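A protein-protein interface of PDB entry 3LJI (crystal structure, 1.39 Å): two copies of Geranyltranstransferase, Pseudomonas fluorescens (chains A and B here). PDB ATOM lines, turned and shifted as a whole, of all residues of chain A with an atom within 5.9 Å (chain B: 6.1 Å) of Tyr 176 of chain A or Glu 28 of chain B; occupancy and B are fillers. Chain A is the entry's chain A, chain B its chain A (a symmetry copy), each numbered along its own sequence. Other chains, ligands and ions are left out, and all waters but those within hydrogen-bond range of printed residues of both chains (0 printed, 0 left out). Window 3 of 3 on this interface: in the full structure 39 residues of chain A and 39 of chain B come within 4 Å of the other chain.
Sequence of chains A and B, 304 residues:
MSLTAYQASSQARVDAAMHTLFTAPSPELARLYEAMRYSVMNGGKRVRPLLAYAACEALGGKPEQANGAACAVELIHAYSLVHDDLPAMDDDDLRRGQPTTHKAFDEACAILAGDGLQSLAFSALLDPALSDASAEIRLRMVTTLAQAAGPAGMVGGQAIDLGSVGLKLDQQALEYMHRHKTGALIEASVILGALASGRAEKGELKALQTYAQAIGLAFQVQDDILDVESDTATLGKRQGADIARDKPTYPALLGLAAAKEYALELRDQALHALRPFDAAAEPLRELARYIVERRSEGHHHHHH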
ATOM      1  N   GLY A 156     -27.023 -10.637 -33.195  1.00  0.00           N
ATOM      2  CA  GLY A 156     -26.745 -12.015 -32.745  1.00  0.00           C
ATOM      3  C   GLY A 156     -28.012 -12.825 -32.516  1.00  0.00           C
ATOM      4  O   GLY A 156     -28.112 -13.983 -32.971  1.00  0.00           O
ATOM      5  N   ALA A 159     -29.538 -13.868 -35.679  1.00  0.00           N
ATOM      6  CA  ALA A 159     -28.768 -14.949 -36.300  1.00  0.00           C
ATOM      7  C   ALA A 159     -29.038 -16.286 -35.616  1.00  0.00           C
ATOM      8  O   ALA A 159     -29.107 -17.324 -36.293  1.00  0.00           O
ATOM      9  CB  ALA A 159     -27.301 -14.625 -36.254  1.00  0.00           C
ATOM     10  N   ILE A 160     -29.202 -16.263 -34.293  1.00  0.00           N
ATOM     11  CA  ILE A 160     -29.554 -17.467 -33.507  1.00  0.00           C
ATOM     12  C   ILE A 160     -30.944 -17.958 -33.923  1.00  0.00           C
ATOM     13  O   ILE A 160     -31.146 -19.158 -34.126  1.00  0.00           O
ATOM     14  CB  ILE A 160     -29.472 -17.228 -31.969  1.00  0.00           C
ATOM     15  CG1 ILE A 160     -28.055 -16.844 -31.551  1.00  0.00           C
ATOM     16  CG2 ILE A 160     -29.902 -18.472 -31.159  1.00  0.00           C
ATOM     17  CD1 ILE A 160     -28.013 -16.034 -30.293  1.00  0.00           C
ATOM     18  N   GLN A 171     -35.937 -24.843 -23.040  1.00  0.00           N
ATOM     19  CA  GLN A 171     -36.188 -23.535 -22.432  1.00  0.00           C
ATOM     20  C   GLN A 171     -34.939 -22.654 -22.368  1.00  0.00           C
ATOM     21  O   GLN A 171     -35.000 -21.476 -22.722  1.00  0.00           O
ATOM     22  CB  GLN A 171     -36.826 -23.689 -21.043  1.00  0.00           C
ATOM     23  CG  GLN A 171     -37.130 -22.348 -20.343  1.00  0.00           C
ATOM     24  CD  GLN A 171     -38.071 -22.487 -19.157  1.00  0.00           C
ATOM     25  OE1 GLN A 171     -38.477 -23.586 -18.792  1.00  0.00           O
ATOM     26  NE2 GLN A 171     -38.421 -21.361 -18.551  1.00  0.00           N
ATOM     27  N   GLN A 172     -33.827 -23.222 -21.913  1.00  0.00           N
ATOM     28  CA  GLN A 172     -32.554 -22.506 -21.827  1.00  0.00           C
ATOM     29  C   GLN A 172     -32.135 -21.917 -23.177  1.00  0.00           C
ATOM     30  O   GLN A 172     -31.692 -20.762 -23.251  1.00  0.00           O
ATOM     31  CB  GLN A 172     -31.463 -23.443 -21.303  1.00  0.00           C
ATOM     32  CG  GLN A 172     -30.114 -22.788 -21.001  1.00  0.00           C
ATOM     33  CD  GLN A 172     -29.021 -23.807 -20.678  1.00  0.00           C
ATOM     34  OE1 GLN A 172     -29.287 -24.868 -20.108  1.00  0.00           O
ATOM     35  NE2 GLN A 172     -27.782 -23.478 -21.041  1.00  0.00           N
ATOM     36  N   ALA A 173     -32.276 -22.710 -24.238  1.00  0.00           N
ATOM     37  CA  ALA A 173     -31.918 -22.271 -25.585  1.00  0.00           C
ATOM     38  C   ALA A 173     -32.865 -21.205 -26.111  1.00  0.00           C
ATOM     39  O   ALA A 173     -32.430 -20.257 -26.764  1.00  0.00           O
ATOM     40  CB  ALA A 173     -31.857 -23.454 -26.557  1.00  0.00           C
ATOM     41  N   LEU A 174     -34.157 -21.379 -25.839  1.00  0.00           N
ATOM     42  CA  LEU A 174     -35.154 -20.398 -26.236  1.00  0.00           C
ATOM     43  C   LEU A 174     -34.895 -19.068 -25.526  1.00  0.00           C
ATOM     44  O   LEU A 174     -34.923 -18.000 -26.163  1.00  0.00           O
ATOM     45  CB  LEU A 174     -36.559 -20.922 -25.933  1.00  0.00           C
ATOM     46  CG  LEU A 174     -37.751 -20.081 -26.383  1.00  0.00           C
ATOM     47  CD1 LEU A 174     -37.771 -19.883 -27.889  1.00  0.00           C
ATOM     48  CD2 LEU A 174     -39.029 -20.760 -25.899  1.00  0.00           C
ATOM     49  N   GLU A 175     -34.607 -19.138 -24.224  1.00  0.00           N
ATOM     50  CA  GLU A 175     -34.350 -17.935 -23.419  1.00  0.00           C
ATOM     51  C   GLU A 175     -33.092 -17.202 -23.902  1.00  0.00           C
ATOM     52  O   GLU A 175     -33.102 -15.983 -24.053  1.00  0.00           O
ATOM     53  CB  GLU A 175     -34.236 -18.297 -21.930  1.00  0.00           C
ATOM     54  CG  GLU A 175     -33.872 -17.125 -21.019  1.00  0.00           C
ATOM     55  CD  GLU A 175     -33.745 -17.520 -19.559  1.00  0.00           C
ATOM     56  OE1 GLU A 175     -34.427 -18.488 -19.138  1.00  0.00           O
ATOM     57  OE2 GLU A 175     -32.970 -16.848 -18.831  1.00  0.00           O
ATOM     58  N   TYR A 176     -32.020 -17.953 -24.150  1.00  0.00           N
ATOM     59  CA  TYR A 176     -30.797 -17.380 -24.700  1.00  0.00           C
ATOM     60  C   TYR A 176     -31.064 -16.585 -25.982  1.00  0.00           C
ATOM     61  O   TYR A 176     -30.616 -15.433 -26.124  1.00  0.00           O
ATOM     62  CB  TYR A 176     -29.787 -18.502 -24.963  1.00  0.00           C
ATOM     63  CG  TYR A 176     -28.468 -18.006 -25.481  1.00  0.00           C
ATOM     64  CD1 TYR A 176     -27.479 -17.565 -24.609  1.00  0.00           C
ATOM     65  CD2 TYR A 176     -28.211 -17.966 -26.849  1.00  0.00           C
ATOM     66  CE1 TYR A 176     -26.256 -17.099 -25.076  1.00  0.00           C
ATOM     67  CE2 TYR A 176     -26.987 -17.500 -27.329  1.00  0.00           C
ATOM     68  CZ  TYR A 176     -26.023 -17.073 -26.434  1.00  0.00           C
ATOM     69  OH  TYR A 176     -24.819 -16.617 -26.924  1.00  0.00           O
ATOM     70  N   MET A 177     -31.796 -17.184 -26.921  1.00  0.00           N
ATOM     71  CA  MET A 177     -32.144 -16.516 -28.166  1.00  0.00           C
ATOM     72  C   MET A 177     -32.937 -15.242 -27.894  1.00  0.00           C
ATOM     73  O   MET A 177     -32.593 -14.187 -28.406  1.00  0.00           O
ATOM     74  CB  MET A 177     -32.943 -17.459 -29.067  1.00  0.00           C
ATOM     75  CG  MET A 177     -33.232 -16.895 -30.442  1.00  0.00           C
ATOM     76  SD  MET A 177     -34.563 -17.969 -31.351  1.00  0.00           S
ATOM     77  CE  MET A 177     -36.059 -17.645 -30.159  1.00  0.00           C
ATOM     78  N   HIS A 178     -33.995 -15.344 -27.089  1.00  0.00           N
ATOM     79  CA  HIS A 178     -34.795 -14.149 -26.760  1.00  0.00           C
ATOM     80  C   HIS A 178     -34.014 -13.059 -26.049  1.00  0.00           C
ATOM     81  O   HIS A 178     -34.192 -11.869 -26.370  1.00  0.00           O
ATOM     82  CB  HIS A 178     -36.036 -14.499 -25.948  1.00  0.00           C
ATOM     83  CG  HIS A 178     -37.089 -15.214 -26.734  1.00  0.00           C
ATOM     84  ND1 HIS A 178     -37.526 -14.784 -27.972  1.00  0.00           N
ATOM     85  CD2 HIS A 178     -37.803 -16.329 -26.446  1.00  0.00           C
ATOM     86  CE1 HIS A 178     -38.447 -15.621 -28.420  1.00  0.00           C
ATOM     87  NE2 HIS A 178     -38.634 -16.562 -27.513  1.00  0.00           N
ATOM     88  N   ARG A 179     -33.167 -13.437 -25.090  1.00  0.00           N
ATOM     89  CA  ARG A 179     -32.350 -12.455 -24.380  1.00  0.00           C
ATOM     90  C   ARG A 179     -31.530 -11.624 -25.362  1.00  0.00           C
ATOM     91  O   ARG A 179     -31.305 -10.421 -25.143  1.00  0.00           O
ATOM     92  CB  ARG A 179     -31.396 -13.119 -23.382  1.00  0.00           C
ATOM     93  CG  ARG A 179     -32.023 -13.584 -22.063  1.00  0.00           C
ATOM     94  CD  ARG A 179     -31.932 -12.514 -20.976  1.00  0.00           C
ATOM     95  NE  ARG A 179     -30.561 -12.064 -20.701  1.00  0.00           N
ATOM     96  CZ  ARG A 179     -29.916 -12.247 -19.547  1.00  0.00           C
ATOM     97  NH1 ARG A 179     -30.508 -12.861 -18.527  1.00  0.00           N
ATOM     98  NH2 ARG A 179     -28.674 -11.796 -19.404  1.00  0.00           N
ATOM     99  N   HIS A 180     -31.065 -12.248 -26.447  1.00  0.00           N
ATOM    100  CA  HIS A 180     -30.326 -11.518 -27.483  1.00  0.00           C
ATOM    101  C   HIS A 180     -31.227 -10.781 -28.460  1.00  0.00           C
ATOM    102  O   HIS A 180     -31.032  -9.582 -28.684  1.00  0.00           O
ATOM    103  CB  HIS A 180     -29.360 -12.477 -28.202  1.00  0.00           C
ATOM    104  CG  HIS A 180     -28.219 -12.915 -27.344  1.00  0.00           C
ATOM    105  ND1 HIS A 180     -28.373 -13.819 -26.314  1.00  0.00           N
ATOM    106  CD2 HIS A 180     -26.912 -12.557 -27.337  1.00  0.00           C
ATOM    107  CE1 HIS A 180     -27.212 -13.991 -25.708  1.00  0.00           C
ATOM    108  NE2 HIS A 180     -26.309 -13.242 -26.312  1.00  0.00           N
ATOM    109  N   LYS A 181     -32.204 -11.479 -29.031  1.00  0.00           N
ATOM    110  CA  LYS A 181     -33.016 -10.920 -30.098  1.00  0.00           C
ATOM    111  C   LYS A 181     -33.801  -9.691 -29.670  1.00  0.00           C
ATOM    112  O   LYS A 181     -33.854  -8.702 -30.423  1.00  0.00           O
ATOM    113  CB  LYS A 181     -33.931 -11.988 -30.709  1.00  0.00           C
ATOM    114  CG  LYS A 181     -34.659 -11.566 -31.966  1.00  0.00           C
ATOM    115  CD  LYS A 181     -35.499 -12.734 -32.484  1.00  0.00           C
ATOM    116  CE  LYS A 181     -36.650 -12.267 -33.370  1.00  0.00           C
ATOM    117  NZ  LYS A 181     -36.497 -12.752 -34.771  1.00  0.00           N
ATOM    118  N   PRO B  25     -18.861 -14.781 -28.890  1.00  0.00           N
ATOM    119  CA  PRO B  25     -18.904 -15.020 -27.445  1.00  0.00           C
ATOM    120  C   PRO B  25     -19.538 -16.358 -27.057  1.00  0.00           C
ATOM    121  O   PRO B  25     -19.482 -16.762 -25.884  1.00  0.00           O
ATOM    122  CB  PRO B  25     -19.705 -13.835 -26.905  1.00  0.00           C
ATOM    123  CG  PRO B  25     -20.477 -13.311 -28.061  1.00  0.00           C
ATOM    124  CD  PRO B  25     -19.779 -13.711 -29.326  1.00  0.00           C
ATOM    125  N   SER B  26     -20.097 -17.064 -28.033  1.00  0.00           N
ATOM    126  CA  SER B  26     -20.720 -18.362 -27.802  1.00  0.00           C
ATOM    127  C   SER B  26     -20.780 -19.177 -29.089  1.00  0.00           C
ATOM    128  O   SER B  26     -20.787 -18.609 -30.179  1.00  0.00           O
ATOM    129  CB  SER B  26     -22.141 -18.179 -27.273  1.00  0.00           C
ATOM    130  OG  SER B  26     -23.003 -17.823 -28.343  1.00  0.00           O
ATOM    131  N   PRO B  27     -20.863 -20.514 -28.980  1.00  0.00           N
ATOM    132  CA  PRO B  27     -20.992 -21.344 -30.186  1.00  0.00           C
ATOM    133  C   PRO B  27     -22.216 -21.013 -31.047  1.00  0.00           C
ATOM    134  O   PRO B  27     -22.155 -21.128 -32.278  1.00  0.00           O
ATOM    135  CB  PRO B  27     -21.088 -22.774 -29.627  1.00  0.00           C
ATOM    136  CG  PRO B  27     -20.429 -22.705 -28.293  1.00  0.00           C
ATOM    137  CD  PRO B  27     -20.706 -21.331 -27.757  1.00  0.00           C
ATOM    138  N   GLU B  28     -23.322 -20.611 -30.412  1.00  0.00           N
ATOM    139  CA  GLU B  28     -24.541 -20.265 -31.128  1.00  0.00           C
ATOM    140  C   GLU B  28     -24.313 -19.109 -32.116  1.00  0.00           C
ATOM    141  O   GLU B  28     -25.046 -18.984 -33.097  1.00  0.00           O
ATOM    142  CB  GLU B  28     -25.659 -19.852 -30.150  1.00  0.00           C
ATOM    143  CG  GLU B  28     -26.206 -20.964 -29.253  1.00  0.00           C
ATOM    144  CD  GLU B  28     -25.468 -21.073 -27.927  1.00  0.00           C
ATOM    145  OE1 GLU B  28     -24.299 -20.641 -27.817  1.00  0.00           O
ATOM    146  OE2 GLU B  28     -26.065 -21.604 -26.967  1.00  0.00           O
ATOM    147  N   LEU B  29     -23.315 -18.271 -31.825  1.00  0.00           N
ATOM    148  CA  LEU B  29     -23.032 -17.088 -32.621  1.00  0.00           C
ATOM    149  C   LEU B  29     -21.878 -17.296 -33.612  1.00  0.00           C
ATOM    150  O   LEU B  29     -21.480 -16.379 -34.335  1.00  0.00           O
ATOM    151  CB  LEU B  29     -22.760 -15.892 -31.703  1.00  0.00           C
ATOM    152  CG  LEU B  29     -23.972 -15.364 -30.932  1.00  0.00           C
ATOM    153  CD1 LEU B  29     -23.546 -14.379 -29.847  1.00  0.00           C
ATOM    154  CD2 LEU B  29     -24.922 -14.706 -31.907  1.00  0.00           C
ATOM    155  N   ALA B  30     -21.357 -18.518 -33.658  1.00  0.00           N
ATOM    156  CA  ALA B  30     -20.166 -18.788 -34.463  1.00  0.00           C
ATOM    157  C   ALA B  30     -20.352 -18.478 -35.950  1.00  0.00           C
ATOM    158  O   ALA B  30     -19.470 -17.860 -36.552  1.00  0.00           O
ATOM    159  CB  ALA B  30     -19.680 -20.229 -34.278  1.00  0.00           C
ATOM    160  N   ARG B  31     -21.485 -18.885 -36.530  1.00  0.00           N
ATOM    161  CA  ARG B  31     -21.699 -18.685 -37.962  1.00  0.00           C
ATOM    162  C   ARG B  31     -21.734 -17.198 -38.303  1.00  0.00           C
ATOM    163  O   ARG B  31     -21.140 -16.784 -39.297  1.00  0.00           O
ATOM    164  CB  ARG B  31     -22.967 -19.397 -38.449  1.00  0.00           C
ATOM    165  CG  ARG B  31     -23.190 -19.314 -39.972  1.00  0.00           C
ATOM    166  CD  ARG B  31     -24.311 -20.276 -40.445  1.00  0.00           C
ATOM    167  NE  ARG B  31     -24.313 -20.470 -41.905  1.00  0.00           N
ATOM    168  CZ  ARG B  31     -25.218 -19.953 -42.731  1.00  0.00           C
ATOM    169  NH1 ARG B  31     -26.199 -19.194 -42.255  1.00  0.00           N
ATOM    170  NH2 ARG B  31     -25.141 -20.174 -44.043  1.00  0.00           N
ATOM    171  N   LEU B  32     -22.415 -16.403 -37.468  1.00  0.00           N
ATOM    172  CA  LEU B  32     -22.488 -14.976 -37.711  1.00  0.00           C
ATOM    173  C   LEU B  32     -21.105 -14.363 -37.703  1.00  0.00           C
ATOM    174  O   LEU B  32     -20.764 -13.595 -38.587  1.00  0.00           O
ATOM    175  CB  LEU B  32     -23.380 -14.268 -36.685  1.00  0.00           C
ATOM    176  CG  LEU B  32     -23.345 -12.728 -36.792  1.00  0.00           C
ATOM    177  CD1 LEU B  32     -23.938 -12.238 -38.116  1.00  0.00           C
ATOM    178  CD2 LEU B  32     -24.141 -12.107 -35.636  1.00  0.00           C
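Hydrophobic or aromatic side chains of chain A within 4 Å of the printed part of chain B: Ala 159, Ile 160 and Tyr 176. Among the printed residues, 7 pairs touch across the chains. Among the printed residues, no Asp or Glu carboxylate lies within 4 Å of a Lys or Arg side-chain nitrogen of the other chain.
No position is printed for both chains.
Of the printed residues of chain B, Ile 160 of chain A touches Leu 29. Of chain B, only Ser 26 (2.6 Å), Glu 28 (3.9 Å) and Leu 29 (3.9 Å) come within 4 Å of Tyr 176 of chain A. Printed residues of chain A within 4 Å of Ser 26 of chain B: Tyr 176 (2.6 Å). Of the printed residues of chain A, Glu 28 of chain B touches Tyr 176 (3.9 Å). Printed residues of chain A within 4 Å of Leu 29 of chain B: Gly 156, Ile 160 and Tyr 176. Printed residues of chain A within 4 Å of Leu 32 of chain B: Gly 156 (3.9 Å) and Ala 159 (3.96 Å). The nearest residue of chain B that does not touch Tyr 176 of chain A is Pro 25 of chain B (5.3 Å). The nearest printed residue of chain A that does not touch Glu 28 of chain B is Ile 160 of chain A (4.003 Å).
The backbone carbonyl oxygen of Tyr 176 of chain A lies within hydrogen-bond range of a ring nitrogen (ND1) of His 180 of chain A (2.8 Å). The side-chain carboxylate (OE1) of Glu 28 of chain B sits at hydrogen-bond distance from the side-chain hydroxyl (OG) of Ser 26 of chain B (3.1 Å).
The side-chain hydroxyl of Tyr 176 of chain A sits at hydrogen-bond distance from the side-chain hydroxyl of Ser 26 of chain B, 2.6 Å away.
Gly 156 of chain A touches Leu 29 of chain B (CA to CD2, 3.4 Å). Leu 32 of chain B touches Gly 156 of chain A. CB of Ala 159 of chain A touches CB of Leu 32 of chain B, 3.96 Å away. Leu 29 of chain B touches Ile 160 of chain A (CD2 to CD1, 3.7 Å). Tyr 176 of chain A touches Glu 28 of chain B. OH of Tyr 176 of chain A touches CD1 of Leu 29 of chain B (3.9 Å).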
